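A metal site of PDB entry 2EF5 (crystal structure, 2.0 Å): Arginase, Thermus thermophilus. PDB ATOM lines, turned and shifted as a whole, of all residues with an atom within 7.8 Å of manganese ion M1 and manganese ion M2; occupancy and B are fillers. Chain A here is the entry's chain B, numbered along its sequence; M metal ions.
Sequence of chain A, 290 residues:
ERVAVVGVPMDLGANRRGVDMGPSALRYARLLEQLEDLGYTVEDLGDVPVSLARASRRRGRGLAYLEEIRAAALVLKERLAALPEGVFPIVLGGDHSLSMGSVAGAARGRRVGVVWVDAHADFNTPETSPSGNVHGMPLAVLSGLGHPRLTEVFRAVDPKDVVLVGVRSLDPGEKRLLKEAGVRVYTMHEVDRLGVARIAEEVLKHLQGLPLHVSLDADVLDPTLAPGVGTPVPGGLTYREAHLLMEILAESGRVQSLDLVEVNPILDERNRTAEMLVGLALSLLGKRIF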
ATOM      1  N   GLY A  94      25.067  28.636   4.706  1.00  0.00           N
ATOM      2  CA  GLY A  94      24.751  27.246   4.866  1.00  0.00           C
ATOM      3  C   GLY A  94      25.204  27.194   6.305  1.00  0.00           C
ATOM      4  O   GLY A  94      24.642  27.901   7.144  1.00  0.00           O
ATOM      5  N   ASP A  95      26.271  26.450   6.567  1.00  0.00           N
ATOM      6  CA  ASP A  95      26.810  26.291   7.916  1.00  0.00           C
ATOM      7  C   ASP A  95      27.085  27.570   8.654  1.00  0.00           C
ATOM      8  O   ASP A  95      27.549  28.557   8.082  1.00  0.00           O
ATOM      9  CB  ASP A  95      28.121  25.487   7.874  1.00  0.00           C
ATOM     10  CG  ASP A  95      27.960  24.150   7.222  1.00  0.00           C
ATOM     11  OD1 ASP A  95      26.908  23.522   7.438  1.00  0.00           O
ATOM     12  OD2 ASP A  95      28.894  23.724   6.512  1.00  0.00           O
ATOM     13  N   HIS A  96      26.836  27.543   9.958  1.00  0.00           N
ATOM     14  CA  HIS A  96      27.104  28.688  10.798  1.00  0.00           C
ATOM     15  C   HIS A  96      28.622  28.869  10.909  1.00  0.00           C
ATOM     16  O   HIS A  96      29.106  29.868  11.425  1.00  0.00           O
ATOM     17  CB  HIS A  96      26.488  28.515  12.190  1.00  0.00           C
ATOM     18  CG  HIS A  96      26.107  29.817  12.838  1.00  0.00           C
ATOM     19  ND1 HIS A  96      25.180  29.907  13.858  1.00  0.00           N
ATOM     20  CD2 HIS A  96      26.498  31.081  12.564  1.00  0.00           C
ATOM     21  CE1 HIS A  96      25.021  31.176  14.180  1.00  0.00           C
ATOM     22  NE2 HIS A  96      25.801  31.915  13.416  1.00  0.00           N
ATOM     23  N   SER A  97      29.365  27.884  10.418  1.00  0.00           N
ATOM     24  CA  SER A  97      30.835  27.947  10.451  1.00  0.00           C
ATOM     25  C   SER A  97      31.346  29.189   9.712  1.00  0.00           C
ATOM     26  O   SER A  97      32.419  29.707  10.023  1.00  0.00           O
ATOM     27  CB  SER A  97      31.445  26.706   9.797  1.00  0.00           C
ATOM     28  OG  SER A  97      31.141  25.535  10.522  1.00  0.00           O
ATOM     29  N   SER A  99      30.530  32.068   9.976  1.00  0.00           N
ATOM     30  CA  SER A  99      30.635  33.227  10.853  1.00  0.00           C
ATOM     31  C   SER A  99      32.056  33.491  11.337  1.00  0.00           C
ATOM     32  O   SER A  99      32.375  34.600  11.728  1.00  0.00           O
ATOM     33  CB  SER A  99      29.683  33.081  12.032  1.00  0.00           C
ATOM     34  OG  SER A  99      28.348  33.260  11.596  1.00  0.00           O
ATOM     35  N   TRP A 116      24.465  36.767  19.076  1.00  0.00           N
ATOM     36  CA  TRP A 116      24.270  35.453  18.473  1.00  0.00           C
ATOM     37  C   TRP A 116      22.862  34.983  18.821  1.00  0.00           C
ATOM     38  O   TRP A 116      22.576  34.635  19.961  1.00  0.00           O
ATOM     39  CB  TRP A 116      25.352  34.515  19.026  1.00  0.00           C
ATOM     40  CG  TRP A 116      25.706  33.292  18.208  1.00  0.00           C
ATOM     41  CD1 TRP A 116      25.147  32.042  18.319  1.00  0.00           C
ATOM     42  CD2 TRP A 116      26.765  33.165  17.249  1.00  0.00           C
ATOM     43  NE1 TRP A 116      25.808  31.155  17.493  1.00  0.00           N
ATOM     44  CE2 TRP A 116      26.797  31.820  16.838  1.00  0.00           C
ATOM     45  CE3 TRP A 116      27.691  34.075  16.710  1.00  0.00           C
ATOM     46  CZ2 TRP A 116      27.734  31.344  15.899  1.00  0.00           C
ATOM     47  CZ3 TRP A 116      28.622  33.600  15.778  1.00  0.00           C
ATOM     48  CH2 TRP A 116      28.633  32.250  15.376  1.00  0.00           C
ATOM     49  N   VAL A 117      21.972  35.012  17.825  1.00  0.00           N
ATOM     50  CA  VAL A 117      20.577  34.631  17.986  1.00  0.00           C
ATOM     51  C   VAL A 117      20.507  33.233  17.411  1.00  0.00           C
ATOM     52  O   VAL A 117      20.486  33.043  16.183  1.00  0.00           O
ATOM     53  CB  VAL A 117      19.676  35.620  17.227  1.00  0.00           C
ATOM     54  CG1 VAL A 117      18.211  35.429  17.611  1.00  0.00           C
ATOM     55  CG2 VAL A 117      20.138  37.050  17.550  1.00  0.00           C
ATOM     56  N   ASP A 118      20.455  32.258  18.309  1.00  0.00           N
ATOM     57  CA  ASP A 118      20.548  30.851  17.934  1.00  0.00           C
ATOM     58  C   ASP A 118      19.932  29.934  18.993  1.00  0.00           C
ATOM     59  O   ASP A 118      19.873  30.311  20.158  1.00  0.00           O
ATOM     60  CB  ASP A 118      22.056  30.554  17.821  1.00  0.00           C
ATOM     61  CG  ASP A 118      22.370  29.376  16.960  1.00  0.00           C
ATOM     62  OD1 ASP A 118      21.666  28.348  17.042  1.00  0.00           O
ATOM     63  OD2 ASP A 118      23.355  29.490  16.191  1.00  0.00           O
ATOM     64  N   ALA A 119      19.462  28.754  18.588  1.00  0.00           N
ATOM     65  CA  ALA A 119      18.912  27.797  19.561  1.00  0.00           C
ATOM     66  C   ALA A 119      20.094  27.150  20.259  1.00  0.00           C
ATOM     67  O   ALA A 119      19.962  26.604  21.352  1.00  0.00           O
ATOM     68  CB  ALA A 119      18.087  26.731  18.848  1.00  0.00           C
ATOM     69  N   HIS A 120      21.254  27.197  19.592  1.00  0.00           N
ATOM     70  CA  HIS A 120      22.491  26.618  20.115  1.00  0.00           C
ATOM     71  C   HIS A 120      23.536  27.694  20.401  1.00  0.00           C
ATOM     72  O   HIS A 120      23.422  28.822  19.929  1.00  0.00           O
ATOM     73  CB  HIS A 120      23.080  25.624  19.116  1.00  0.00           C
ATOM     74  CG  HIS A 120      22.110  24.570  18.666  1.00  0.00           C
ATOM     75  ND1 HIS A 120      21.304  24.730  17.560  1.00  0.00           N
ATOM     76  CD2 HIS A 120      21.801  23.363  19.195  1.00  0.00           C
ATOM     77  CE1 HIS A 120      20.540  23.661  17.419  1.00  0.00           C
ATOM     78  NE2 HIS A 120      20.820  22.812  18.404  1.00  0.00           N
ATOM     79  N   ALA A 121      24.566  27.338  21.153  1.00  0.00           N
ATOM     80  CA  ALA A 121      25.607  28.296  21.499  1.00  0.00           C
ATOM     81  C   ALA A 121      26.810  28.239  20.561  1.00  0.00           C
ATOM     82  O   ALA A 121      27.597  29.188  20.511  1.00  0.00           O
ATOM     83  CB  ALA A 121      26.049  28.081  22.925  1.00  0.00           C
ATOM     84  N   ASP A 122      26.963  27.140  19.832  1.00  0.00           N
ATOM     85  CA  ASP A 122      28.088  26.986  18.924  1.00  0.00           C
ATOM     86  C   ASP A 122      29.377  27.347  19.636  1.00  0.00           C
ATOM     87  O   ASP A 122      30.273  27.978  19.047  1.00  0.00           O
ATOM     88  CB  ASP A 122      27.917  27.878  17.693  1.00  0.00           C
ATOM     89  CG  ASP A 122      26.702  27.507  16.873  1.00  0.00           C
ATOM     90  OD1 ASP A 122      26.435  26.301  16.735  1.00  0.00           O
ATOM     91  OD2 ASP A 122      26.029  28.425  16.366  1.00  0.00           O
ATOM     92  N   HIS A 135      30.720  23.434  12.510  1.00  0.00           N
ATOM     93  CA  HIS A 135      29.643  24.415  12.596  1.00  0.00           C
ATOM     94  C   HIS A 135      29.030  24.493  13.987  1.00  0.00           C
ATOM     95  O   HIS A 135      28.069  25.226  14.218  1.00  0.00           O
ATOM     96  CB  HIS A 135      28.564  24.147  11.525  1.00  0.00           C
ATOM     97  CG  HIS A 135      28.060  22.740  11.505  1.00  0.00           C
ATOM     98  ND1 HIS A 135      27.333  22.191  12.542  1.00  0.00           N
ATOM     99  CD2 HIS A 135      28.128  21.783  10.545  1.00  0.00           C
ATOM    100  CE1 HIS A 135      26.977  20.953  12.223  1.00  0.00           C
ATOM    101  NE2 HIS A 135      27.445  20.692  11.012  1.00  0.00           N
ATOM    102  N   GLY A 136      29.610  23.739  14.921  1.00  0.00           N
ATOM    103  CA  GLY A 136      29.133  23.762  16.294  1.00  0.00           C
ATOM    104  C   GLY A 136      30.189  24.425  17.176  1.00  0.00           C
ATOM    105  O   GLY A 136      30.074  24.419  18.398  1.00  0.00           O
ATOM    106  N   MET A 137      31.208  25.005  16.542  1.00  0.00           N
ATOM    107  CA  MET A 137      32.298  25.666  17.276  1.00  0.00           C
ATOM    108  C   MET A 137      32.676  27.087  16.825  1.00  0.00           C
ATOM    109  O   MET A 137      33.585  27.677  17.391  1.00  0.00           O
ATOM    110  CB  MET A 137      33.588  24.819  17.176  1.00  0.00           C
ATOM    111  CG  MET A 137      33.412  23.340  16.867  1.00  0.00           C
ATOM    112  SD  MET A 137      35.000  22.488  16.512  1.00  0.00           S
ATOM    113  CE  MET A 137      34.676  20.881  17.278  1.00  0.00           C
ATOM    114  N   PRO A 138      31.983  27.660  15.825  1.00  0.00           N
ATOM    115  CA  PRO A 138      32.372  29.021  15.390  1.00  0.00           C
ATOM    116  C   PRO A 138      32.420  30.150  16.421  1.00  0.00           C
ATOM    117  O   PRO A 138      33.324  30.988  16.380  1.00  0.00           O
ATOM    118  CB  PRO A 138      31.378  29.311  14.260  1.00  0.00           C
ATOM    119  CG  PRO A 138      30.163  28.551  14.677  1.00  0.00           C
ATOM    120  CD  PRO A 138      30.750  27.232  15.144  1.00  0.00           C
ATOM    121  N   LEU A 139      31.454  30.188  17.337  1.00  0.00           N
ATOM    122  CA  LEU A 139      31.466  31.245  18.339  1.00  0.00           C
ATOM    123  C   LEU A 139      32.625  31.064  19.313  1.00  0.00           C
ATOM    124  O   LEU A 139      33.185  32.038  19.807  1.00  0.00           O
ATOM    125  CB  LEU A 139      30.134  31.289  19.098  1.00  0.00           C
ATOM    126  CG  LEU A 139      30.005  32.469  20.066  1.00  0.00           C
ATOM    127  CD1 LEU A 139      30.319  33.774  19.327  1.00  0.00           C
ATOM    128  CD2 LEU A 139      28.604  32.512  20.661  1.00  0.00           C
ATOM    129  N   SER A 169      19.449  24.580  23.788  1.00  0.00           N
ATOM    130  CA  SER A 169      20.127  23.292  23.688  1.00  0.00           C
ATOM    131  C   SER A 169      21.638  23.473  23.807  1.00  0.00           C
ATOM    132  O   SER A 169      22.263  24.132  22.970  1.00  0.00           O
ATOM    133  CB  SER A 169      19.800  22.617  22.355  1.00  0.00           C
ATOM    134  OG  SER A 169      20.396  21.341  22.259  1.00  0.00           O
ATOM    135  N   SER A 215      24.269  37.724  14.261  1.00  0.00           N
ATOM    136  CA  SER A 215      24.361  36.447  13.556  1.00  0.00           C
ATOM    137  C   SER A 215      23.067  35.733  13.880  1.00  0.00           C
ATOM    138  O   SER A 215      22.843  35.326  15.015  1.00  0.00           O
ATOM    139  CB  SER A 215      25.559  35.638  14.060  1.00  0.00           C
ATOM    140  OG  SER A 215      25.810  34.526  13.217  1.00  0.00           O
ATOM    141  N   LEU A 216      22.223  35.591  12.871  1.00  0.00           N
ATOM    142  CA  LEU A 216      20.914  34.969  13.035  1.00  0.00           C
ATOM    143  C   LEU A 216      20.837  33.589  12.410  1.00  0.00           C
ATOM    144  O   LEU A 216      20.916  33.442  11.192  1.00  0.00           O
ATOM    145  CB  LEU A 216      19.852  35.893  12.417  1.00  0.00           C
ATOM    146  CG  LEU A 216      18.384  35.442  12.402  1.00  0.00           C
ATOM    147  CD1 LEU A 216      17.890  35.206  13.820  1.00  0.00           C
ATOM    148  CD2 LEU A 216      17.550  36.517  11.715  1.00  0.00           C
ATOM    149  N   ASP A 217      20.693  32.580  13.264  1.00  0.00           N
ATOM    150  CA  ASP A 217      20.567  31.192  12.871  1.00  0.00           C
ATOM    151  C   ASP A 217      19.060  30.949  12.816  1.00  0.00           C
ATOM    152  O   ASP A 217      18.347  31.248  13.775  1.00  0.00           O
ATOM    153  CB  ASP A 217      21.216  30.278  13.924  1.00  0.00           C
ATOM    154  CG  ASP A 217      21.218  28.815  13.507  1.00  0.00           C
ATOM    155  OD1 ASP A 217      20.184  28.325  13.008  1.00  0.00           O
ATOM    156  OD2 ASP A 217      22.256  28.131  13.680  1.00  0.00           O
ATOM    157  N   ALA A 218      18.586  30.424  11.706  1.00  0.00           N
ATOM    158  CA  ALA A 218      17.153  30.186  11.527  1.00  0.00           C
ATOM    159  C   ALA A 218      16.552  29.314  12.611  1.00  0.00           C
ATOM    160  O   ALA A 218      15.363  29.444  12.945  1.00  0.00           O
ATOM    161  CB  ALA A 218      16.895  29.568  10.144  1.00  0.00           C
ATOM    162  N   ASP A 219      17.347  28.424  13.192  1.00  0.00           N
ATOM    163  CA  ASP A 219      16.798  27.529  14.188  1.00  0.00           C
ATOM    164  C   ASP A 219      16.414  28.179  15.508  1.00  0.00           C
ATOM    165  O   ASP A 219      15.860  27.509  16.372  1.00  0.00           O
ATOM    166  CB  ASP A 219      17.737  26.331  14.444  1.00  0.00           C
ATOM    167  CG  ASP A 219      18.986  26.700  15.228  1.00  0.00           C
ATOM    168  OD1 ASP A 219      19.078  27.803  15.790  1.00  0.00           O
ATOM    169  OD2 ASP A 219      19.898  25.848  15.279  1.00  0.00           O
ATOM    170  N   VAL A 220      16.675  29.478  15.662  1.00  0.00           N
ATOM    171  CA  VAL A 220      16.273  30.128  16.908  1.00  0.00           C
ATOM    172  C   VAL A 220      14.753  30.225  16.940  1.00  0.00           C
ATOM    173  O   VAL A 220      14.131  30.231  18.008  1.00  0.00           O
ATOM    174  CB  VAL A 220      16.893  31.561  17.050  1.00  0.00           C
ATOM    175  CG1 VAL A 220      16.236  32.543  16.081  1.00  0.00           C
ATOM    176  CG2 VAL A 220      16.752  32.025  18.491  1.00  0.00           C
ATOM    177  N   VAL A 229      15.389  23.813   8.973  1.00  0.00           N
ATOM    178  CA  VAL A 229      16.643  23.927   9.698  1.00  0.00           C
ATOM    179  C   VAL A 229      17.169  22.520  10.015  1.00  0.00           C
ATOM    180  O   VAL A 229      16.390  21.606  10.280  1.00  0.00           O
ATOM    181  CB  VAL A 229      16.475  24.711  11.019  1.00  0.00           C
ATOM    182  CG1 VAL A 229      15.921  26.106  10.730  1.00  0.00           C
ATOM    183  CG2 VAL A 229      15.548  23.960  11.962  1.00  0.00           C
ATOM    184  N   THR A 231      18.996  21.352  12.663  1.00  0.00           N
ATOM    185  CA  THR A 231      18.816  20.882  14.026  1.00  0.00           C
ATOM    186  C   THR A 231      17.687  21.608  14.734  1.00  0.00           C
ATOM    187  O   THR A 231      17.923  22.494  15.561  1.00  0.00           O
ATOM    188  CB  THR A 231      20.118  21.048  14.847  1.00  0.00           C
ATOM    189  OG1 THR A 231      21.222  20.565  14.083  1.00  0.00           O
ATOM    190  CG2 THR A 231      20.028  20.246  16.139  1.00  0.00           C
ATOM    191  N   VAL A 233      14.790  22.569  17.323  1.00  0.00           N
ATOM    192  CA  VAL A 233      14.607  22.373  18.758  1.00  0.00           C
ATOM    193  C   VAL A 233      13.314  23.072  19.158  1.00  0.00           C
ATOM    194  O   VAL A 233      13.168  24.286  18.983  1.00  0.00           O
ATOM    195  CB  VAL A 233      15.771  22.975  19.568  1.00  0.00           C
ATOM    196  CG1 VAL A 233      15.662  22.553  21.022  1.00  0.00           C
ATOM    197  CG2 VAL A 233      17.112  22.525  18.988  1.00  0.00           C
ATOM    198  N   VAL A 261      21.952  32.517   8.562  1.00  0.00           N
ATOM    199  CA  VAL A 261      22.459  31.181   8.371  1.00  0.00           C
ATOM    200  C   VAL A 261      21.563  30.010   8.681  1.00  0.00           C
ATOM    201  O   VAL A 261      20.494  30.163   9.266  1.00  0.00           O
ATOM    202  CB  VAL A 261      23.757  30.989   9.202  1.00  0.00           C
ATOM    203  CG1 VAL A 261      24.754  32.091   8.856  1.00  0.00           C
ATOM    204  CG2 VAL A 261      23.419  31.034  10.693  1.00  0.00           C
ATOM    205  N   GLU A 262      22.028  28.831   8.270  1.00  0.00           N
ATOM    206  CA  GLU A 262      21.374  27.556   8.514  1.00  0.00           C
ATOM    207  C   GLU A 262      20.012  27.317   7.862  1.00  0.00           C
ATOM    208  O   GLU A 262      19.250  26.461   8.306  1.00  0.00           O
ATOM    209  CB  GLU A 262      21.279  27.322  10.024  1.00  0.00           C
ATOM    210  CG  GLU A 262      22.627  27.167  10.719  1.00  0.00           C
ATOM    211  CD  GLU A 262      23.291  25.814  10.445  1.00  0.00           C
ATOM    212  OE1 GLU A 262      22.588  24.786  10.526  1.00  0.00           O
ATOM    213  OE2 GLU A 262      24.508  25.769  10.173  1.00  0.00           O
HETATM  214 MN    MN M   1      21.953  26.644  15.749  1.00  0.00          MN
HETATM  215 MN    MN M   2      24.360  28.197  14.905  1.00  0.00          MN
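The backbone NH (N) of His 120 lies close to the side-chain carboxylate (OD1) of Asp 118. The indole nitrogen (NE1) of Trp 116 lies close to the side-chain carboxylate (OD2) of Asp 118. OG of Ser 215 sits at hydrogen-bond distance from NE2 of His 96, at 2.6 Å. OG of Ser 99 lies close to NE2 of His 96, at 3.4 Å. The backbone carbonyl oxygen (O) of Asp 122 sits at hydrogen-bond distance from the backbone NH (N) of Leu 139 (3.0 Å). The side-chain carboxylate of Asp 219 lies close to a ring nitrogen (ND1) of His 120 (2.9 Å). The backbone NH (N) of Ala 119 sits at hydrogen-bond distance from the side-chain carboxylate (OD1) of Asp 219, 3.0 Å away. The backbone NH of Asp 217 sits at hydrogen-bond distance from the backbone carbonyl oxygen of Val 117 (3.0 Å).
Four residues have an atom within 4 Å of manganese ion M1: Asp 118, His 120, Asp 217 and Asp 219. Along chain A the residues within 4 Å of manganese ion M1 span positions 118 to 219.
Within 4 Å of manganese ion M2: His 96, Asp 118, Asp 122 and Asp 217. The nearest printed residue that does not touch manganese ion M2 is Trp 116 (4.2 Å).
Manganese ion M1 is bound by OD1 of Asp 118 (2.2 Å), OD2 of Asp 219 (2.3 Å) and OD2 of Asp 217 (2.6 Å). Manganese ion M1 has three donor atoms within binding distance. Slightly farther from manganese ion M1 lies a ring nitrogen (ND1) of His 120 (2.7 Å).
Manganese ion M2 is bound by the side-chain carboxylate (OD2) of Asp 118 (2.1 Å), a ring nitrogen (ND1) of His 96 (2.2 Å), the side-chain carboxylate (OD2) of Asp 122 (2.2 Å) and the side-chain carboxylate (OD2) of Asp 217 (2.4 Å).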
